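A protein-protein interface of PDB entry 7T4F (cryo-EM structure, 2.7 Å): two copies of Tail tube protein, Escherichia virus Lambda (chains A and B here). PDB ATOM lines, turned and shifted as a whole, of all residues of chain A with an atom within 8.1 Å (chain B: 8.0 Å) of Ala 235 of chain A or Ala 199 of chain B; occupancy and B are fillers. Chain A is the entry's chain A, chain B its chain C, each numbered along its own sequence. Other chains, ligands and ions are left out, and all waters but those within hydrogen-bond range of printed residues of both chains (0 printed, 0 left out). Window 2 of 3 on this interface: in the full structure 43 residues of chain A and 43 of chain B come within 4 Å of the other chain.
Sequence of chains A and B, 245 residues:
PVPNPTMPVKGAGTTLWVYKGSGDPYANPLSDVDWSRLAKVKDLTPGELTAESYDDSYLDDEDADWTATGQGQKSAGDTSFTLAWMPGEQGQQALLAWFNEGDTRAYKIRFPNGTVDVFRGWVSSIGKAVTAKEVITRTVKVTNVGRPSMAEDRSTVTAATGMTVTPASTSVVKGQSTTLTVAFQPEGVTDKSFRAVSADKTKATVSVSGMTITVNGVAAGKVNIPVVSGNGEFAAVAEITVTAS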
ATOM      1  N   GLY A 162      20.189  -4.473 -19.524  1.00  0.00           N
ATOM      2  CA  GLY A 162      19.772  -3.895 -20.787  1.00  0.00           C
ATOM      3  C   GLY A 162      18.500  -3.095 -20.639  1.00  0.00           C
ATOM      4  O   GLY A 162      17.764  -3.230 -19.656  1.00  0.00           O
ATOM      5  N   MET A 163      18.248  -2.254 -21.639  1.00  0.00           N
ATOM      6  CA  MET A 163      17.066  -1.404 -21.691  1.00  0.00           C
ATOM      7  C   MET A 163      16.344  -1.631 -23.011  1.00  0.00           C
ATOM      8  O   MET A 163      16.972  -1.638 -24.074  1.00  0.00           O
ATOM      9  CB  MET A 163      17.446   0.072 -21.536  1.00  0.00           C
ATOM     10  CG  MET A 163      16.274   1.037 -21.620  1.00  0.00           C
ATOM     11  SD  MET A 163      16.706   2.692 -21.047  1.00  0.00           S
ATOM     12  CE  MET A 163      15.082   3.420 -20.848  1.00  0.00           C
ATOM     13  N   THR A 164      15.027  -1.813 -22.940  1.00  0.00           N
ATOM     14  CA  THR A 164      14.206  -2.078 -24.114  1.00  0.00           C
ATOM     15  C   THR A 164      13.027  -1.116 -24.152  1.00  0.00           C
ATOM     16  O   THR A 164      12.424  -0.815 -23.117  1.00  0.00           O
ATOM     17  CB  THR A 164      13.691  -3.526 -24.127  1.00  0.00           C
ATOM     18  OG1 THR A 164      12.903  -3.767 -22.954  1.00  0.00           O
ATOM     19  CG2 THR A 164      14.851  -4.510 -24.168  1.00  0.00           C
ATOM     20  N   VAL A 165      12.706  -0.638 -25.351  1.00  0.00           N
ATOM     21  CA  VAL A 165      11.536   0.199 -25.595  1.00  0.00           C
ATOM     22  C   VAL A 165      10.583  -0.572 -26.499  1.00  0.00           C
ATOM     23  O   VAL A 165      11.006  -1.171 -27.496  1.00  0.00           O
ATOM     24  CB  VAL A 165      11.922   1.562 -26.203  1.00  0.00           C
ATOM     25  CG1 VAL A 165      12.595   1.397 -27.562  1.00  0.00           C
ATOM     26  CG2 VAL A 165      10.697   2.460 -26.318  1.00  0.00           C
ATOM     27  N   PRO A 226      15.219   9.183 -29.795  1.00  0.00           N
ATOM     28  CA  PRO A 226      16.187   8.466 -28.957  1.00  0.00           C
ATOM     29  C   PRO A 226      15.807   8.517 -27.486  1.00  0.00           C
ATOM     30  O   PRO A 226      15.295   9.523 -26.989  1.00  0.00           O
ATOM     31  CB  PRO A 226      17.501   9.214 -29.213  1.00  0.00           C
ATOM     32  CG  PRO A 226      17.077  10.587 -29.602  1.00  0.00           C
ATOM     33  CD  PRO A 226      15.773  10.435 -30.341  1.00  0.00           C
ATOM     34  N   VAL A 227      16.079   7.418 -26.787  1.00  0.00           N
ATOM     35  CA  VAL A 227      15.883   7.320 -25.346  1.00  0.00           C
ATOM     36  C   VAL A 227      17.208   6.910 -24.717  1.00  0.00           C
ATOM     37  O   VAL A 227      17.812   5.909 -25.122  1.00  0.00           O
ATOM     38  CB  VAL A 227      14.770   6.322 -24.987  1.00  0.00           C
ATOM     39  CG1 VAL A 227      14.760   6.051 -23.489  1.00  0.00           C
ATOM     40  CG2 VAL A 227      13.422   6.850 -25.446  1.00  0.00           C
ATOM     41  N   VAL A 228      17.656   7.679 -23.727  1.00  0.00           N
ATOM     42  CA  VAL A 228      18.926   7.443 -23.053  1.00  0.00           C
ATOM     43  C   VAL A 228      18.669   7.323 -21.558  1.00  0.00           C
ATOM     44  O   VAL A 228      17.918   8.119 -20.983  1.00  0.00           O
ATOM     45  CB  VAL A 228      19.945   8.565 -23.345  1.00  0.00           C
ATOM     46  CG1 VAL A 228      21.261   8.296 -22.627  1.00  0.00           C
ATOM     47  CG2 VAL A 228      20.169   8.699 -24.842  1.00  0.00           C
ATOM     48  N   SER A 229      19.293   6.327 -20.934  1.00  0.00           N
ATOM     49  CA  SER A 229      19.133   6.113 -19.504  1.00  0.00           C
ATOM     50  C   SER A 229      19.772   7.250 -18.714  1.00  0.00           C
ATOM     51  O   SER A 229      20.634   7.979 -19.214  1.00  0.00           O
ATOM     52  CB  SER A 229      19.753   4.777 -19.093  1.00  0.00           C
ATOM     53  OG  SER A 229      21.153   4.774 -19.314  1.00  0.00           O
ATOM     54  N   ASN A 231      21.824   7.087 -16.185  1.00  0.00           N
ATOM     55  CA  ASN A 231      23.286   6.874 -16.019  1.00  0.00           C
ATOM     56  C   ASN A 231      23.979   7.103 -17.361  1.00  0.00           C
ATOM     57  O   ASN A 231      25.168   7.446 -17.354  1.00  0.00           O
ATOM     58  CB  ASN A 231      23.608   5.483 -15.471  1.00  0.00           C
ATOM     59  CG  ASN A 231      23.012   4.359 -16.292  1.00  0.00           C
ATOM     60  OD1 ASN A 231      22.827   4.490 -17.499  1.00  0.00           O
ATOM     61  ND2 ASN A 231      22.719   3.244 -15.645  1.00  0.00           N
ATOM     62  N   GLY A 232      23.260   6.888 -18.466  1.00  0.00           N
ATOM     63  CA  GLY A 232      23.839   7.058 -19.780  1.00  0.00           C
ATOM     64  C   GLY A 232      24.658   5.890 -20.280  1.00  0.00           C
ATOM     65  O   GLY A 232      25.441   6.064 -21.222  1.00  0.00           O
ATOM     66  N   GLU A 233      24.517   4.707 -19.681  1.00  0.00           N
ATOM     67  CA  GLU A 233      25.320   3.575 -20.125  1.00  0.00           C
ATOM     68  C   GLU A 233      24.596   2.791 -21.216  1.00  0.00           C
ATOM     69  O   GLU A 233      25.235   2.138 -22.047  1.00  0.00           O
ATOM     70  CB  GLU A 233      25.667   2.682 -18.932  1.00  0.00           C
ATOM     71  CG  GLU A 233      26.760   1.650 -19.198  1.00  0.00           C
ATOM     72  CD  GLU A 233      26.249   0.381 -19.842  1.00  0.00           C
ATOM     73  OE1 GLU A 233      25.076   0.035 -19.622  1.00  0.00           O
ATOM     74  OE2 GLU A 233      27.025  -0.271 -20.573  1.00  0.00           O
ATOM     75  N   PHE A 234      23.264   2.858 -21.241  1.00  0.00           N
ATOM     76  CA  PHE A 234      22.463   2.235 -22.285  1.00  0.00           C
ATOM     77  C   PHE A 234      21.810   3.307 -23.146  1.00  0.00           C
ATOM     78  O   PHE A 234      21.732   4.478 -22.759  1.00  0.00           O
ATOM     79  CB  PHE A 234      21.357   1.321 -21.727  1.00  0.00           C
ATOM     80  CG  PHE A 234      21.808   0.383 -20.645  1.00  0.00           C
ATOM     81  CD1 PHE A 234      21.945   0.814 -19.334  1.00  0.00           C
ATOM     82  CD2 PHE A 234      22.086  -0.941 -20.940  1.00  0.00           C
ATOM     83  CE1 PHE A 234      22.347  -0.060 -18.341  1.00  0.00           C
ATOM     84  CE2 PHE A 234      22.495  -1.816 -19.955  1.00  0.00           C
ATOM     85  CZ  PHE A 234      22.623  -1.377 -18.653  1.00  0.00           C
ATOM     86  N   ALA A 235      21.338   2.892 -24.321  1.00  0.00           N
ATOM     87  CA  ALA A 235      20.627   3.774 -25.235  1.00  0.00           C
ATOM     88  C   ALA A 235      19.607   2.967 -26.024  1.00  0.00           C
ATOM     89  O   ALA A 235      19.850   1.810 -26.374  1.00  0.00           O
ATOM     90  CB  ALA A 235      21.588   4.485 -26.194  1.00  0.00           C
ATOM     91  N   ALA A 236      18.465   3.591 -26.305  1.00  0.00           N
ATOM     92  CA  ALA A 236      17.410   2.986 -27.106  1.00  0.00           C
ATOM     93  C   ALA A 236      16.893   4.014 -28.101  1.00  0.00           C
ATOM     94  O   ALA A 236      16.624   5.161 -27.731  1.00  0.00           O
ATOM     95  CB  ALA A 236      16.266   2.471 -26.227  1.00  0.00           C
ATOM     96  N   VAL A 237      16.756   3.603 -29.359  1.00  0.00           N
ATOM     97  CA  VAL A 237      16.290   4.473 -30.432  1.00  0.00           C
ATOM     98  C   VAL A 237      14.981   3.918 -30.972  1.00  0.00           C
ATOM     99  O   VAL A 237      14.915   2.755 -31.390  1.00  0.00           O
ATOM    100  CB  VAL A 237      17.338   4.600 -31.550  1.00  0.00           C
ATOM    101  CG1 VAL A 237      16.799   5.451 -32.690  1.00  0.00           C
ATOM    102  CG2 VAL A 237      18.628   5.191 -31.001  1.00  0.00           C
ATOM    103  N   ALA A 238      13.941   4.747 -30.964  1.00  0.00           N
ATOM    104  CA  ALA A 238      12.627   4.377 -31.473  1.00  0.00           C
ATOM    105  C   ALA A 238      12.288   5.248 -32.674  1.00  0.00           C
ATOM    106  O   ALA A 238      12.337   6.480 -32.587  1.00  0.00           O
ATOM    107  CB  ALA A 238      11.558   4.523 -30.389  1.00  0.00           C
ATOM    108  N   ALA B 196      27.081  11.110 -25.795  1.00  0.00           N
ATOM    109  CA  ALA B 196      26.872  10.292 -27.010  1.00  0.00           C
ATOM    110  C   ALA B 196      26.932   8.828 -26.595  1.00  0.00           C
ATOM    111  O   ALA B 196      27.970   8.411 -26.058  1.00  0.00           O
ATOM    112  CB  ALA B 196      27.926  10.617 -28.031  1.00  0.00           C
ATOM    113  N   VAL B 197      25.867   8.074 -26.857  1.00  0.00           N
ATOM    114  CA  VAL B 197      25.828   6.680 -26.333  1.00  0.00           C
ATOM    115  C   VAL B 197      25.622   5.700 -27.477  1.00  0.00           C
ATOM    116  O   VAL B 197      25.268   6.139 -28.584  1.00  0.00           O
ATOM    117  CB  VAL B 197      24.735   6.511 -25.263  1.00  0.00           C
ATOM    118  CG1 VAL B 197      25.188   7.066 -23.925  1.00  0.00           C
ATOM    119  CG2 VAL B 197      23.436   7.171 -25.694  1.00  0.00           C
ATOM    120  N   SER B 198      25.851   4.424 -27.198  1.00  0.00           N
ATOM    121  CA  SER B 198      25.698   3.375 -28.198  1.00  0.00           C
ATOM    122  C   SER B 198      24.493   2.506 -27.868  1.00  0.00           C
ATOM    123  O   SER B 198      24.339   2.049 -26.731  1.00  0.00           O
ATOM    124  CB  SER B 198      26.960   2.515 -28.274  1.00  0.00           C
ATOM    125  OG  SER B 198      26.800   1.458 -29.204  1.00  0.00           O
ATOM    126  N   ALA B 199      23.635   2.284 -28.867  1.00  0.00           N
ATOM    127  CA  ALA B 199      22.497   1.390 -28.676  1.00  0.00           C
ATOM    128  C   ALA B 199      22.954  -0.048 -28.471  1.00  0.00           C
ATOM    129  O   ALA B 199      22.419  -0.762 -27.614  1.00  0.00           O
ATOM    130  CB  ALA B 199      21.545   1.486 -29.869  1.00  0.00           C
ATOM    131  N   ASP B 200      23.943  -0.491 -29.245  1.00  0.00           N
ATOM    132  CA  ASP B 200      24.473  -1.847 -29.160  1.00  0.00           C
ATOM    133  C   ASP B 200      25.975  -1.764 -28.927  1.00  0.00           C
ATOM    134  O   ASP B 200      26.724  -1.360 -29.822  1.00  0.00           O
ATOM    135  CB  ASP B 200      24.158  -2.637 -30.431  1.00  0.00           C
ATOM    136  CG  ASP B 200      22.679  -2.936 -30.578  1.00  0.00           C
ATOM    137  OD1 ASP B 200      21.990  -3.054 -29.544  1.00  0.00           O
ATOM    138  OD2 ASP B 200      22.205  -3.053 -31.726  1.00  0.00           O
ATOM    139  N   LYS B 201      26.411  -2.162 -27.731  1.00  0.00           N
ATOM    140  CA  LYS B 201      27.850  -2.026 -27.389  1.00  0.00           C
ATOM    141  C   LYS B 201      28.671  -3.077 -28.149  1.00  0.00           C
ATOM    142  O   LYS B 201      29.808  -2.760 -28.537  1.00  0.00           O
ATOM    143  CB  LYS B 201      28.060  -2.123 -25.875  1.00  0.00           C
ATOM    144  CG  LYS B 201      29.440  -1.700 -25.390  1.00  0.00           C
ATOM    145  CD  LYS B 201      29.467  -1.281 -23.938  1.00  0.00           C
ATOM    146  CE  LYS B 201      28.998  -2.365 -22.994  1.00  0.00           C
ATOM    147  NZ  LYS B 201      29.075  -1.926 -21.581  1.00  0.00           N
ATOM    148  N   THR B 202      28.125  -4.278 -28.355  1.00  0.00           N
ATOM    149  CA  THR B 202      28.859  -5.299 -29.094  1.00  0.00           C
ATOM    150  C   THR B 202      29.089  -4.871 -30.537  1.00  0.00           C
ATOM    151  O   THR B 202      30.168  -5.093 -31.098  1.00  0.00           O
ATOM    152  CB  THR B 202      28.108  -6.630 -29.038  1.00  0.00           C
ATOM    153  OG1 THR B 202      26.826  -6.483 -29.664  1.00  0.00           O
ATOM    154  CG2 THR B 202      27.916  -7.071 -27.595  1.00  0.00           C
ATOM    155  N   LYS B 203      28.079  -4.259 -31.158  1.00  0.00           N
ATOM    156  CA  LYS B 203      28.201  -3.872 -32.558  1.00  0.00           C
ATOM    157  C   LYS B 203      29.146  -2.686 -32.729  1.00  0.00           C
ATOM    158  O   LYS B 203      29.901  -2.624 -33.706  1.00  0.00           O
ATOM    159  CB  LYS B 203      26.819  -3.557 -33.129  1.00  0.00           C
ATOM    160  CG  LYS B 203      25.923  -4.783 -33.248  1.00  0.00           C
ATOM    161  CD  LYS B 203      24.538  -4.420 -33.750  1.00  0.00           C
ATOM    162  CE  LYS B 203      24.581  -4.017 -35.208  1.00  0.00           C
ATOM    163  NZ  LYS B 203      24.920  -5.181 -36.072  1.00  0.00           N
ATOM    164  N   ALA B 204      29.124  -1.741 -31.789  1.00  0.00           N
ATOM    165  CA  ALA B 204      29.999  -0.580 -31.855  1.00  0.00           C
ATOM    166  C   ALA B 204      30.171   0.012 -30.463  1.00  0.00           C
ATOM    167  O   ALA B 204      29.307  -0.140 -29.595  1.00  0.00           O
ATOM    168  CB  ALA B 204      29.452   0.486 -32.812  1.00  0.00           C
ATOM    169  N   THR B 205      31.298   0.694 -30.263  1.00  0.00           N
ATOM    170  CA  THR B 205      31.597   1.393 -29.020  1.00  0.00           C
ATOM    171  C   THR B 205      32.011   2.822 -29.342  1.00  0.00           C
ATOM    172  O   THR B 205      32.592   3.083 -30.399  1.00  0.00           O
ATOM    173  CB  THR B 205      32.708   0.691 -28.228  1.00  0.00           C
ATOM    174  OG1 THR B 205      33.896   0.615 -29.028  1.00  0.00           O
ATOM    175  CG2 THR B 205      32.278  -0.713 -27.826  1.00  0.00           C
ATOM    176  N   VAL B 206      31.715   3.742 -28.427  1.00  0.00           N
ATOM    177  CA  VAL B 206      31.955   5.166 -28.634  1.00  0.00           C
ATOM    178  C   VAL B 206      32.790   5.707 -27.482  1.00  0.00           C
ATOM    179  O   VAL B 206      32.570   5.345 -26.320  1.00  0.00           O
ATOM    180  CB  VAL B 206      30.636   5.952 -28.771  1.00  0.00           C
ATOM    181  CG1 VAL B 206      29.981   5.654 -30.110  1.00  0.00           C
ATOM    182  CG2 VAL B 206      29.694   5.617 -27.626  1.00  0.00           C
ATOM    183  N   LYS B 222      24.495  -2.866 -38.755  1.00  0.00           N
ATOM    184  CA  LYS B 222      23.963  -1.509 -38.691  1.00  0.00           C
ATOM    185  C   LYS B 222      23.665  -1.156 -37.241  1.00  0.00           C
ATOM    186  O   LYS B 222      22.844  -1.813 -36.593  1.00  0.00           O
ATOM    187  CB  LYS B 222      22.696  -1.376 -39.538  1.00  0.00           C
ATOM    188  CG  LYS B 222      22.527  -0.019 -40.207  1.00  0.00           C
ATOM    189  CD  LYS B 222      21.123   0.148 -40.771  1.00  0.00           C
ATOM    190  CE  LYS B 222      20.882  -0.770 -41.958  1.00  0.00           C
ATOM    191  NZ  LYS B 222      19.459  -0.729 -42.399  1.00  0.00           N
ATOM    192  N   VAL B 223      24.316  -0.107 -36.742  1.00  0.00           N
ATOM    193  CA  VAL B 223      24.183   0.322 -35.356  1.00  0.00           C
ATOM    194  C   VAL B 223      23.844   1.806 -35.333  1.00  0.00           C
ATOM    195  O   VAL B 223      24.423   2.597 -36.087  1.00  0.00           O
ATOM    196  CB  VAL B 223      25.464   0.032 -34.546  1.00  0.00           C
ATOM    197  CG1 VAL B 223      26.682   0.637 -35.229  1.00  0.00           C
ATOM    198  CG2 VAL B 223      25.328   0.548 -33.118  1.00  0.00           C
ATOM    199  N   ASN B 224      22.897   2.176 -34.475  1.00  0.00           N
ATOM    200  CA  ASN B 224      22.490   3.563 -34.305  1.00  0.00           C
ATOM    201  C   ASN B 224      23.215   4.147 -33.098  1.00  0.00           C
ATOM    202  O   ASN B 224      23.223   3.541 -32.020  1.00  0.00           O
ATOM    203  CB  ASN B 224      20.977   3.666 -34.120  1.00  0.00           C
ATOM    204  CG  ASN B 224      20.250   3.988 -35.410  1.00  0.00           C
ATOM    205  OD1 ASN B 224      20.764   4.710 -36.265  1.00  0.00           O
ATOM    206  ND2 ASN B 224      19.042   3.459 -35.552  1.00  0.00           N
ATOM    207  N   ILE B 225      23.815   5.316 -33.280  1.00  0.00           N
ATOM    208  CA  ILE B 225      24.549   6.008 -32.226  1.00  0.00           C
ATOM    209  C   ILE B 225      23.840   7.328 -31.942  1.00  0.00           C
ATOM    210  O   ILE B 225      24.099   8.334 -32.612  1.00  0.00           O
ATOM    211  CB  ILE B 225      26.017   6.241 -32.621  1.00  0.00           C
ATOM    212  CG1 ILE B 225      26.713   4.910 -32.911  1.00  0.00           C
ATOM    213  CG2 ILE B 225      26.756   6.992 -31.520  1.00  0.00           C
ATOM    214  CD1 ILE B 225      26.749   3.970 -31.729  1.00  0.00           C
ATOM    215  N   PRO B 226      22.960   7.362 -30.907  1.00  0.00           N
ATOM    216  CA  PRO B 226      22.254   8.583 -30.520  1.00  0.00           C
ATOM    217  C   PRO B 226      23.110   9.521 -29.663  1.00  0.00           C
ATOM    218  O   PRO B 226      23.774   9.040 -28.769  1.00  0.00           O
ATOM    219  CB  PRO B 226      21.113   8.051 -29.647  1.00  0.00           C
ATOM    220  CG  PRO B 226      21.700   6.835 -28.983  1.00  0.00           C
ATOM    221  CD  PRO B 226      22.577   6.225 -30.054  1.00  0.00           C
ATOM    222  N   VAL B 227      23.085  10.821 -29.963  1.00  0.00           N
ATOM    223  CA  VAL B 227      23.817  11.825 -29.137  1.00  0.00           C
ATOM    224  C   VAL B 227      22.776  12.791 -28.580  1.00  0.00           C
ATOM    225  O   VAL B 227      21.982  13.324 -29.375  1.00  0.00           O
ATOM    226  CB  VAL B 227      24.863  12.584 -29.968  1.00  0.00           C
ATOM    227  CG1 VAL B 227      25.640  13.575 -29.117  1.00  0.00           C
ATOM    228  CG2 VAL B 227      25.809  11.634 -30.685  1.00  0.00           C
ATOM    229  N   VAL B 228      22.783  13.001 -27.268  1.00  0.00           N
ATOM    230  CA  VAL B 228      21.810  13.934 -26.642  1.00  0.00           C
ATOM    231  C   VAL B 228      22.604  15.052 -25.969  1.00  0.00           C
ATOM    232  O   VAL B 228      23.588  14.737 -25.278  1.00  0.00           O
ATOM    233  CB  VAL B 228      20.896  13.197 -25.649  1.00  0.00           C
ATOM    234  CG1 VAL B 228      19.891  14.139 -25.008  1.00  0.00           C
ATOM    235  CG2 VAL B 228      20.185  12.026 -26.306  1.00  0.00           C
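The side-chain carboxylate of Glu 233 of chain A lies within salt-bridge range of the side-chain amino group of Lys 201 of chain B (2.8 Å).
The backbone carbonyl oxygen (O) of Pro 226 of chain B sits at hydrogen-bond distance from the backbone NH (N) of Val 197 of chain B (3.0 Å). The backbone NH of Ala 199 of chain B sits close to the backbone carbonyl oxygen of Asn 224 of chain B (3.4 Å). The backbone carbonyl oxygen of Asp 200 of chain B lies within hydrogen-bond range of the side-chain hydroxyl of Ser 198 of chain B (2.9 Å). The side-chain hydroxyl (OG) of Ser 229 of chain A is in hydrogen-bond range of the backbone NH (N) of Glu 233 of chain A, 3.4 Å away. The side-chain hydroxyl (OG) of Ser 198 of chain B sits at hydrogen-bond distance from the backbone carbonyl oxygen (O) of Ala 204 of chain B (3.0 Å). The side-chain amide oxygen of Asn 231 of chain A lies within hydrogen-bond range of the backbone NH of Glu 233 of chain A.
Pro 226 of chain B touches Pro 226 of chain A (CB to CB, 3.8 Å). Val 197 of chain B touches Val 228 of chain A (CG2 to CG2, 3.7 Å). CG2 of Val 228 of chain B touches CG2 of Val 228 of chain A, at 3.6 Å. Val 197 of chain B touches Gly 232 of chain A. Ala 235 of chain A touches Val 197 of chain B (CB to CG2, 3.3 Å). Ala 235 of chain A touches Ser 198 of chain B. CA of Ala 199 of chain B touches O of Ala 235 of chain A (3.5 Å). Pro 226 of chain B touches Ala 235 of chain A (CG to CB, 3.6 Å).
Ala 235 of chain A touches just these residues of chain B: Val 197, Ser 198, Ala 199 and Pro 226. Ser 198 of chain B touches just one residue of chain A: Ala 235. Of the printed residues of chain A, Pro 226 of chain B touches Pro 226 (3.8 Å) and Ala 235 (3.6 Å). Of the printed residues of chain B, Glu 233 of chain A touches Lys 201. Of the printed residues of chain B, Gly 232 of chain A touches Val 197. The nearest residue of chain B that does not touch Ala 235 of chain A is Asp 200 of chain B (5.5 Å). The nearest residue of chain A that does not touch Ala 199 of chain B is Val 237 of chain A (4.8 Å).
Of the 18 printed residues of chain B, 6 touch a printed residue of chain A. Hydrophobic or aromatic side chains of chain B within 4 Å of the printed part of chain A: Val 197, Ala 199, Pro 226 and Val 228. Of the 16 printed residues of chain A, 5 touch a printed residue of chain B. Printed residues of chain A that touch a printed residue of chain B: Pro 226, Val 228, Gly 232, Glu 233 and Ala 235. Among the printed residues, 9 pairs touch across the chains.
Pro 226 of chain B touches its own counterpart, Pro 226 of chain A. Val 228 of chain A touches its own counterpart, Val 228 of chain B.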
